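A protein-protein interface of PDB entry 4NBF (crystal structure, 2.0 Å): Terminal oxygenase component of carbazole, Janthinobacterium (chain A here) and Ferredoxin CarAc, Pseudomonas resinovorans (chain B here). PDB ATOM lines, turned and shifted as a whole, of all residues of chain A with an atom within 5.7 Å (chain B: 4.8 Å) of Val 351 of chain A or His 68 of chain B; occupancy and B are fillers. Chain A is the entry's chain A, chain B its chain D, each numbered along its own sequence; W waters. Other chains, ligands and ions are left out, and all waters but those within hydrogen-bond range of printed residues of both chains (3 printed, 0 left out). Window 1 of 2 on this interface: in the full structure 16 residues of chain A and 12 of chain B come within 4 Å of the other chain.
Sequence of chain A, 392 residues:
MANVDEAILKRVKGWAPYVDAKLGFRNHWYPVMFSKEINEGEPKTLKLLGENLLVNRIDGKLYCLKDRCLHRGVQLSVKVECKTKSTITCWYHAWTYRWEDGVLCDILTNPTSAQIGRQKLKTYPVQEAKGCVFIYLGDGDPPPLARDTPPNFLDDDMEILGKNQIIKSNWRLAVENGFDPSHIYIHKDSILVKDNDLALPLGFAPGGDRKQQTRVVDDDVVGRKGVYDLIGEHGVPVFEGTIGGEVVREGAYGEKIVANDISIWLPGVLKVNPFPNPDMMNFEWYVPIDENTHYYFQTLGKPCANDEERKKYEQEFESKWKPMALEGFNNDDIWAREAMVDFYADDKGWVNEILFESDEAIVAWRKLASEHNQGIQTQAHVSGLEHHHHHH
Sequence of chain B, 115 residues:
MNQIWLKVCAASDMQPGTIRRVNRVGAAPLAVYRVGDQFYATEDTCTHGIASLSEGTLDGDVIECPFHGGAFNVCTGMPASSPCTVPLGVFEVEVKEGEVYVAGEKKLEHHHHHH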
ATOM      1  N   ILE A   8      29.338  28.188 -19.617  1.00  0.00           N
ATOM      2  CA  ILE A   8      28.435  27.230 -18.993  1.00  0.00           C
ATOM      3  C   ILE A   8      28.810  27.031 -17.527  1.00  0.00           C
ATOM      4  O   ILE A   8      27.942  27.020 -16.653  1.00  0.00           O
ATOM      5  CB  ILE A   8      28.479  25.869 -19.728  1.00  0.00           C
ATOM      6  CG1 ILE A   8      27.904  26.033 -21.140  1.00  0.00           C
ATOM      7  CG2 ILE A   8      27.700  24.819 -18.940  1.00  0.00           C
ATOM      8  CD1 ILE A   8      28.116  24.836 -22.043  1.00  0.00           C
ATOM      9  N   ARG A  11      27.554  29.650 -15.259  1.00  0.00           N
ATOM     10  CA  ARG A  11      26.124  29.575 -14.962  1.00  0.00           C
ATOM     11  C   ARG A  11      25.756  28.603 -13.844  1.00  0.00           C
ATOM     12  O   ARG A  11      24.861  28.880 -13.047  1.00  0.00           O
ATOM     13  CB  ARG A  11      25.345  29.185 -16.222  1.00  0.00           C
ATOM     14  CG  ARG A  11      24.923  30.353 -17.092  1.00  0.00           C
ATOM     15  CD  ARG A  11      24.350  29.867 -18.418  1.00  0.00           C
ATOM     16  NE  ARG A  11      23.712  30.950 -19.159  1.00  0.00           N
ATOM     17  CZ  ARG A  11      22.508  31.440 -18.882  1.00  0.00           C
ATOM     18  NH1 ARG A  11      21.795  30.939 -17.881  1.00  0.00           N
ATOM     19  NH2 ARG A  11      22.024  32.449 -19.597  1.00  0.00           N
ATOM     20  N   VAL A  12      26.436  27.463 -13.797  1.00  0.00           N
ATOM     21  CA  VAL A  12      26.148  26.455 -12.784  1.00  0.00           C
ATOM     22  C   VAL A  12      26.996  26.659 -11.539  1.00  0.00           C
ATOM     23  O   VAL A  12      27.894  25.874 -11.244  1.00  0.00           O
ATOM     24  CB  VAL A  12      26.367  25.032 -13.355  1.00  0.00           C
ATOM     25  CG1 VAL A  12      25.296  24.733 -14.394  1.00  0.00           C
ATOM     26  CG2 VAL A  12      27.744  24.920 -13.991  1.00  0.00           C
ATOM     27  N   TRP A  15      27.421  23.851  -8.687  1.00  0.00           N
ATOM     28  CA  TRP A  15      28.234  22.654  -8.873  1.00  0.00           C
ATOM     29  C   TRP A  15      29.113  22.651 -10.124  1.00  0.00           C
ATOM     30  O   TRP A  15      29.159  21.657 -10.863  1.00  0.00           O
ATOM     31  CB  TRP A  15      27.308  21.434  -8.865  1.00  0.00           C
ATOM     32  CG  TRP A  15      26.090  21.570  -9.762  1.00  0.00           C
ATOM     33  CD1 TRP A  15      26.045  21.394 -11.114  1.00  0.00           C
ATOM     34  CD2 TRP A  15      24.750  21.897  -9.356  1.00  0.00           C
ATOM     35  NE1 TRP A  15      24.760  21.585 -11.577  1.00  0.00           N
ATOM     36  CE2 TRP A  15      23.948  21.896 -10.518  1.00  0.00           C
ATOM     37  CE3 TRP A  15      24.152  22.188  -8.121  1.00  0.00           C
ATOM     38  CZ2 TRP A  15      22.573  22.174 -10.484  1.00  0.00           C
ATOM     39  CZ3 TRP A  15      22.786  22.466  -8.089  1.00  0.00           C
ATOM     40  CH2 TRP A  15      22.012  22.456  -9.263  1.00  0.00           C
ATOM     41  N   ASP A 347      26.822  19.730 -23.384  1.00  0.00           N
ATOM     42  CA  ASP A 347      26.937  20.378 -22.078  1.00  0.00           C
ATOM     43  C   ASP A 347      25.806  21.371 -21.780  1.00  0.00           C
ATOM     44  O   ASP A 347      25.770  21.964 -20.701  1.00  0.00           O
ATOM     45  CB  ASP A 347      28.294  21.089 -21.936  1.00  0.00           C
ATOM     46  CG  ASP A 347      29.466  20.120 -21.913  1.00  0.00           C
ATOM     47  OD1 ASP A 347      29.390  19.111 -21.180  1.00  0.00           O
ATOM     48  OD2 ASP A 347      30.469  20.366 -22.616  1.00  0.00           O
ATOM     49  N   LYS A 348      24.874  21.537 -22.715  1.00  0.00           N
ATOM     50  CA  LYS A 348      23.765  22.472 -22.517  1.00  0.00           C
ATOM     51  C   LYS A 348      22.658  21.931 -21.601  1.00  0.00           C
ATOM     52  O   LYS A 348      21.911  22.703 -21.004  1.00  0.00           O
ATOM     53  CB  LYS A 348      23.175  22.894 -23.872  1.00  0.00           C
ATOM     54  CG  LYS A 348      24.166  23.635 -24.785  1.00  0.00           C
ATOM     55  CD  LYS A 348      24.666  24.926 -24.145  1.00  0.00           C
ATOM     56  CE  LYS A 348      25.731  25.632 -24.998  1.00  0.00           C
ATOM     57  NZ  LYS A 348      25.222  26.117 -26.316  1.00  0.00           N
ATOM     58  N   GLY A 349      22.555  20.610 -21.486  1.00  0.00           N
ATOM     59  CA  GLY A 349      21.542  20.030 -20.616  1.00  0.00           C
ATOM     60  C   GLY A 349      21.754  20.441 -19.166  1.00  0.00           C
ATOM     61  O   GLY A 349      20.809  20.515 -18.382  1.00  0.00           O
ATOM     62  N   TRP A 350      23.006  20.707 -18.801  1.00  0.00           N
ATOM     63  CA  TRP A 350      23.330  21.121 -17.441  1.00  0.00           C
ATOM     64  C   TRP A 350      22.723  22.487 -17.134  1.00  0.00           C
ATOM     65  O   TRP A 350      22.676  22.905 -15.977  1.00  0.00           O
ATOM     66  CB  TRP A 350      24.851  21.185 -17.245  1.00  0.00           C
ATOM     67  CG  TRP A 350      25.529  19.869 -17.451  1.00  0.00           C
ATOM     68  CD1 TRP A 350      26.373  19.530 -18.469  1.00  0.00           C
ATOM     69  CD2 TRP A 350      25.419  18.712 -16.616  1.00  0.00           C
ATOM     70  NE1 TRP A 350      26.801  18.228 -18.320  1.00  0.00           N
ATOM     71  CE2 TRP A 350      26.229  17.704 -17.190  1.00  0.00           C
ATOM     72  CE3 TRP A 350      24.713  18.427 -15.437  1.00  0.00           C
ATOM     73  CZ2 TRP A 350      26.353  16.429 -16.624  1.00  0.00           C
ATOM     74  CZ3 TRP A 350      24.837  17.155 -14.876  1.00  0.00           C
ATOM     75  CH2 TRP A 350      25.652  16.176 -15.472  1.00  0.00           C
ATOM     76  N   VAL A 351      22.279  23.190 -18.172  1.00  0.00           N
ATOM     77  CA  VAL A 351      21.657  24.499 -17.988  1.00  0.00           C
ATOM     78  C   VAL A 351      20.147  24.448 -18.267  1.00  0.00           C
ATOM     79  O   VAL A 351      19.353  25.055 -17.545  1.00  0.00           O
ATOM     80  CB  VAL A 351      22.278  25.568 -18.933  1.00  0.00           C
ATOM     81  CG1 VAL A 351      21.447  26.837 -18.903  1.00  0.00           C
ATOM     82  CG2 VAL A 351      23.713  25.887 -18.507  1.00  0.00           C
ATOM     83  N   ASN A 352      19.755  23.697 -19.293  1.00  0.00           N
ATOM     84  CA  ASN A 352      18.349  23.634 -19.693  1.00  0.00           C
ATOM     85  C   ASN A 352      17.414  22.631 -19.010  1.00  0.00           C
ATOM     86  O   ASN A 352      16.196  22.702 -19.194  1.00  0.00           O
ATOM     87  CB  ASN A 352      18.271  23.462 -21.211  1.00  0.00           C
ATOM     88  CG  ASN A 352      18.874  24.640 -21.953  1.00  0.00           C
ATOM     89  OD1 ASN A 352      18.561  25.789 -21.654  1.00  0.00           O
ATOM     90  ND2 ASN A 352      19.743  24.361 -22.922  1.00  0.00           N
ATOM     91  N   GLU A 353      17.971  21.707 -18.235  1.00  0.00           N
ATOM     92  CA  GLU A 353      17.165  20.721 -17.515  1.00  0.00           C
ATOM     93  C   GLU A 353      16.139  21.443 -16.635  1.00  0.00           C
ATOM     94  O   GLU A 353      16.421  22.517 -16.109  1.00  0.00           O
ATOM     95  CB  GLU A 353      18.075  19.880 -16.611  1.00  0.00           C
ATOM     96  CG  GLU A 353      18.917  20.746 -15.661  1.00  0.00           C
ATOM     97  CD  GLU A 353      19.922  19.965 -14.823  1.00  0.00           C
ATOM     98  OE1 GLU A 353      20.235  18.803 -15.167  1.00  0.00           O
ATOM     99  OE2 GLU A 353      20.415  20.532 -13.820  1.00  0.00           O
ATOM    100  N   LEU A 355      14.280  20.645 -13.356  1.00  0.00           N
ATOM    101  CA  LEU A 355      14.192  19.724 -12.230  1.00  0.00           C
ATOM    102  C   LEU A 355      12.917  19.855 -11.408  1.00  0.00           C
ATOM    103  O   LEU A 355      12.270  20.901 -11.416  1.00  0.00           O
ATOM    104  CB  LEU A 355      15.395  19.939 -11.306  1.00  0.00           C
ATOM    105  CG  LEU A 355      16.765  20.026 -11.987  1.00  0.00           C
ATOM    106  CD1 LEU A 355      17.847  20.223 -10.939  1.00  0.00           C
ATOM    107  CD2 LEU A 355      17.018  18.764 -12.793  1.00  0.00           C
ATOM    108  N   ARG A 366      25.380  16.444  -6.513  1.00  0.00           N
ATOM    109  CA  ARG A 366      26.201  17.330  -7.329  1.00  0.00           C
ATOM    110  C   ARG A 366      27.027  18.277  -6.454  1.00  0.00           C
ATOM    111  O   ARG A 366      28.210  18.519  -6.721  1.00  0.00           O
ATOM    112  CB  ARG A 366      25.322  18.121  -8.297  1.00  0.00           C
ATOM    113  CG  ARG A 366      24.616  17.259  -9.344  1.00  0.00           C
ATOM    114  CD  ARG A 366      23.778  18.133 -10.262  1.00  0.00           C
ATOM    115  NE  ARG A 366      23.124  17.399 -11.345  1.00  0.00           N
ATOM    116  CZ  ARG A 366      22.251  17.952 -12.180  1.00  0.00           C
ATOM    117  NH1 ARG A 366      21.941  19.237 -12.044  1.00  0.00           N
ATOM    118  NH2 ARG A 366      21.692  17.230 -13.148  1.00  0.00           N
ATOM    119  N   HIS B  48      12.083  27.786 -12.942  1.00  0.00           N
ATOM    120  CA  HIS B  48      12.749  26.838 -13.837  1.00  0.00           C
ATOM    121  C   HIS B  48      13.153  25.527 -13.158  1.00  0.00           C
ATOM    122  O   HIS B  48      13.545  24.572 -13.830  1.00  0.00           O
ATOM    123  CB  HIS B  48      13.978  27.511 -14.464  1.00  0.00           C
ATOM    124  CG  HIS B  48      14.782  26.616 -15.355  1.00  0.00           C
ATOM    125  ND1 HIS B  48      16.038  26.164 -15.014  1.00  0.00           N
ATOM    126  CD2 HIS B  48      14.519  26.105 -16.583  1.00  0.00           C
ATOM    127  CE1 HIS B  48      16.517  25.417 -15.995  1.00  0.00           C
ATOM    128  NE2 HIS B  48      15.615  25.366 -16.959  1.00  0.00           N
ATOM    129  N   CYS B  65      19.423  33.205 -10.656  1.00  0.00           N
ATOM    130  CA  CYS B  65      19.305  31.907  -9.998  1.00  0.00           C
ATOM    131  C   CYS B  65      20.660  31.206  -9.904  1.00  0.00           C
ATOM    132  O   CYS B  65      21.404  31.143 -10.878  1.00  0.00           O
ATOM    133  CB  CYS B  65      18.326  31.030 -10.773  1.00  0.00           C
ATOM    134  SG  CYS B  65      18.191  29.365 -10.137  1.00  0.00           S
ATOM    135  N   PRO B  66      20.984  30.647  -8.725  1.00  0.00           N
ATOM    136  CA  PRO B  66      22.256  29.954  -8.503  1.00  0.00           C
ATOM    137  C   PRO B  66      22.432  28.638  -9.256  1.00  0.00           C
ATOM    138  O   PRO B  66      23.560  28.195  -9.479  1.00  0.00           O
ATOM    139  CB  PRO B  66      22.268  29.753  -6.990  1.00  0.00           C
ATOM    140  CG  PRO B  66      20.828  29.528  -6.690  1.00  0.00           C
ATOM    141  CD  PRO B  66      20.162  30.619  -7.503  1.00  0.00           C
ATOM    142  N   PHE B  67      21.322  28.020  -9.653  1.00  0.00           N
ATOM    143  CA  PHE B  67      21.378  26.743 -10.356  1.00  0.00           C
ATOM    144  C   PHE B  67      21.888  26.804 -11.790  1.00  0.00           C
ATOM    145  O   PHE B  67      22.902  26.184 -12.121  1.00  0.00           O
ATOM    146  CB  PHE B  67      19.995  26.072 -10.360  1.00  0.00           C
ATOM    147  CG  PHE B  67      19.730  25.190  -9.164  1.00  0.00           C
ATOM    148  CD1 PHE B  67      20.377  25.409  -7.951  1.00  0.00           C
ATOM    149  CD2 PHE B  67      18.783  24.172  -9.239  1.00  0.00           C
ATOM    150  CE1 PHE B  67      20.085  24.626  -6.826  1.00  0.00           C
ATOM    151  CE2 PHE B  67      18.482  23.385  -8.120  1.00  0.00           C
ATOM    152  CZ  PHE B  67      19.134  23.616  -6.914  1.00  0.00           C
ATOM    153  N   HIS B  68      21.191  27.547 -12.645  1.00  0.00           N
ATOM    154  CA  HIS B  68      21.581  27.604 -14.051  1.00  0.00           C
ATOM    155  C   HIS B  68      21.830  28.993 -14.626  1.00  0.00           C
ATOM    156  O   HIS B  68      22.081  29.129 -15.820  1.00  0.00           O
ATOM    157  CB  HIS B  68      20.522  26.890 -14.891  1.00  0.00           C
ATOM    158  CG  HIS B  68      20.143  25.542 -14.361  1.00  0.00           C
ATOM    159  ND1 HIS B  68      18.910  25.281 -13.803  1.00  0.00           N
ATOM    160  CD2 HIS B  68      20.834  24.379 -14.304  1.00  0.00           C
ATOM    161  CE1 HIS B  68      18.856  24.014 -13.428  1.00  0.00           C
ATOM    162  NE2 HIS B  68      20.012  23.445 -13.723  1.00  0.00           N
ATOM    163  N   GLY B  69      21.756  30.022 -13.790  1.00  0.00           N
ATOM    164  CA  GLY B  69      22.006  31.365 -14.284  1.00  0.00           C
ATOM    165  C   GLY B  69      20.797  32.066 -14.873  1.00  0.00           C
ATOM    166  O   GLY B  69      20.924  33.145 -15.461  1.00  0.00           O
ATOM    167  N   GLY B  70      19.626  31.450 -14.749  1.00  0.00           N
ATOM    168  CA  GLY B  70      18.419  32.094 -15.242  1.00  0.00           C
ATOM    169  C   GLY B  70      18.201  33.310 -14.357  1.00  0.00           C
ATOM    170  O   GLY B  70      18.765  33.378 -13.263  1.00  0.00           O
ATOM    171  N   PRO B  83      17.767  30.164 -18.759  1.00  0.00           N
ATOM    172  CA  PRO B  83      16.696  29.374 -19.376  1.00  0.00           C
ATOM    173  C   PRO B  83      15.283  29.656 -18.865  1.00  0.00           C
ATOM    174  O   PRO B  83      14.323  29.057 -19.346  1.00  0.00           O
ATOM    175  CB  PRO B  83      17.125  27.943 -19.077  1.00  0.00           C
ATOM    176  CG  PRO B  83      17.683  28.082 -17.690  1.00  0.00           C
ATOM    177  CD  PRO B  83      18.530  29.344 -17.798  1.00  0.00           C
HETATM  178  O   HOH W   1      14.896  25.137 -19.947  1.00  0.00           O
HETATM  179  O   HOH W   2      15.910  23.089 -13.509  1.00  0.00           O
HETATM  180  O   HOH W   3      24.112  31.151 -11.856  1.00  0.00           O
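O of Gly 70 of chain B sits at hydrogen-bond distance from N of Cys 65 of chain B (2.7 Å). OE2 of Glu 353 of chain A lies within salt-bridge range of NH1 of Arg 366 of chain A. SG of Cys 65 of chain B lies close to N of Phe 67 of chain B (3.4 Å). The side-chain amide nitrogen of Asn 352 of chain A sits at hydrogen-bond distance from the backbone carbonyl oxygen of Lys 348 of chain A (3.3 Å).
Among the printed residues, pairs that only touch across the chains: Arg 11 of chain A with Pro 66 of chain B, Arg 11 of chain A with Gly 70 of chain B, Arg 11 of chain A with Pro 83 of chain B, Val 12 of chain A with Phe 67 of chain B, Trp 15 of chain A with Phe 67 of chain B, Trp 350 of chain A with His 68 of chain B, Val 351 of chain A with His 48 of chain B, Val 351 of chain A with His 68 of chain B, Val 351 of chain A with Pro 83 of chain B, Asn 352 of chain A with His 48 of chain B and Asn 352 of chain A with Pro 83 of chain B.
Hydrophobic or aromatic side chains of chain B that line the printed part of chain A: His 48, Phe 67, His 68 and Pro 83. Among the printed residues, no Asp or Glu carboxylate lies within 4 Å of a Lys or Arg side-chain nitrogen of the other chain.
Water W3 lies within hydrogen-bond range of the backbone carbonyl oxygen of Arg 11 of chain A, the backbone carbonyl oxygen of Cys 65 of chain B and the backbone NH of Gly 69 of chain B. Water W2 lies within hydrogen-bond range of the backbone carbonyl oxygen of Glu 353 of chain A (2.7 Å), the backbone carbonyl oxygen of His 48 of chain B (2.8 Å) and the backbone NH of Leu 355 of chain A (2.9 Å). Water W1 bridges the backbone carbonyl oxygen of Asn 352 of chain A (2.9 Å) and a ring nitrogen (NE2) of His 48 of chain B (3.1 Å).
The backbone carbonyl oxygen (O) of Glu 353 of chain A sits close to a ring nitrogen (NE2) of His 48 of chain B (3.1 Å). The backbone carbonyl oxygen (O) of Arg 11 of chain A lies close to the backbone carbonyl oxygen (O) of Phe 67 of chain B (3.5 Å). The guanidinium group (NH1) of Arg 11 of chain A sits close to the backbone carbonyl oxygen (O) of Gly 69 of chain B. OE2 of Glu 353 of chain A lies within hydrogen-bond range of NE2 of His 68 of chain B (2.9 Å). NH1 of Arg 11 of chain A lies within hydrogen-bond range of O of His 68 of chain B, 2.8 Å away.
Of the printed residues of chain B, Arg 11 of chain A touches Pro 66, Phe 67, His 68, Gly 69, Gly 70 and Pro 83. Printed residues of chain B within 4 Å of Trp 350 of chain A: His 68. Of chain B, only His 48 (3.3 Å), His 68 (3.3 Å) and Pro 83 (3.5 Å) come within 4 Å of Val 351 of chain A. Of the printed residues of chain B, Glu 353 of chain A touches His 48 (2.9 Å) and His 68 (2.9 Å). His 68 of chain B touches four residues of chain A. The nearest printed residue of chain B that does not touch Val 351 of chain A is Gly 69 of chain B (6.0 Å). The nearest residue of chain A that does not touch His 68 of chain B is Trp 15 of chain A (4.3 Å). The nearest printed residue of chain B that does not touch Glu 353 of chain A is Pro 83 of chain B (5.9 Å).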
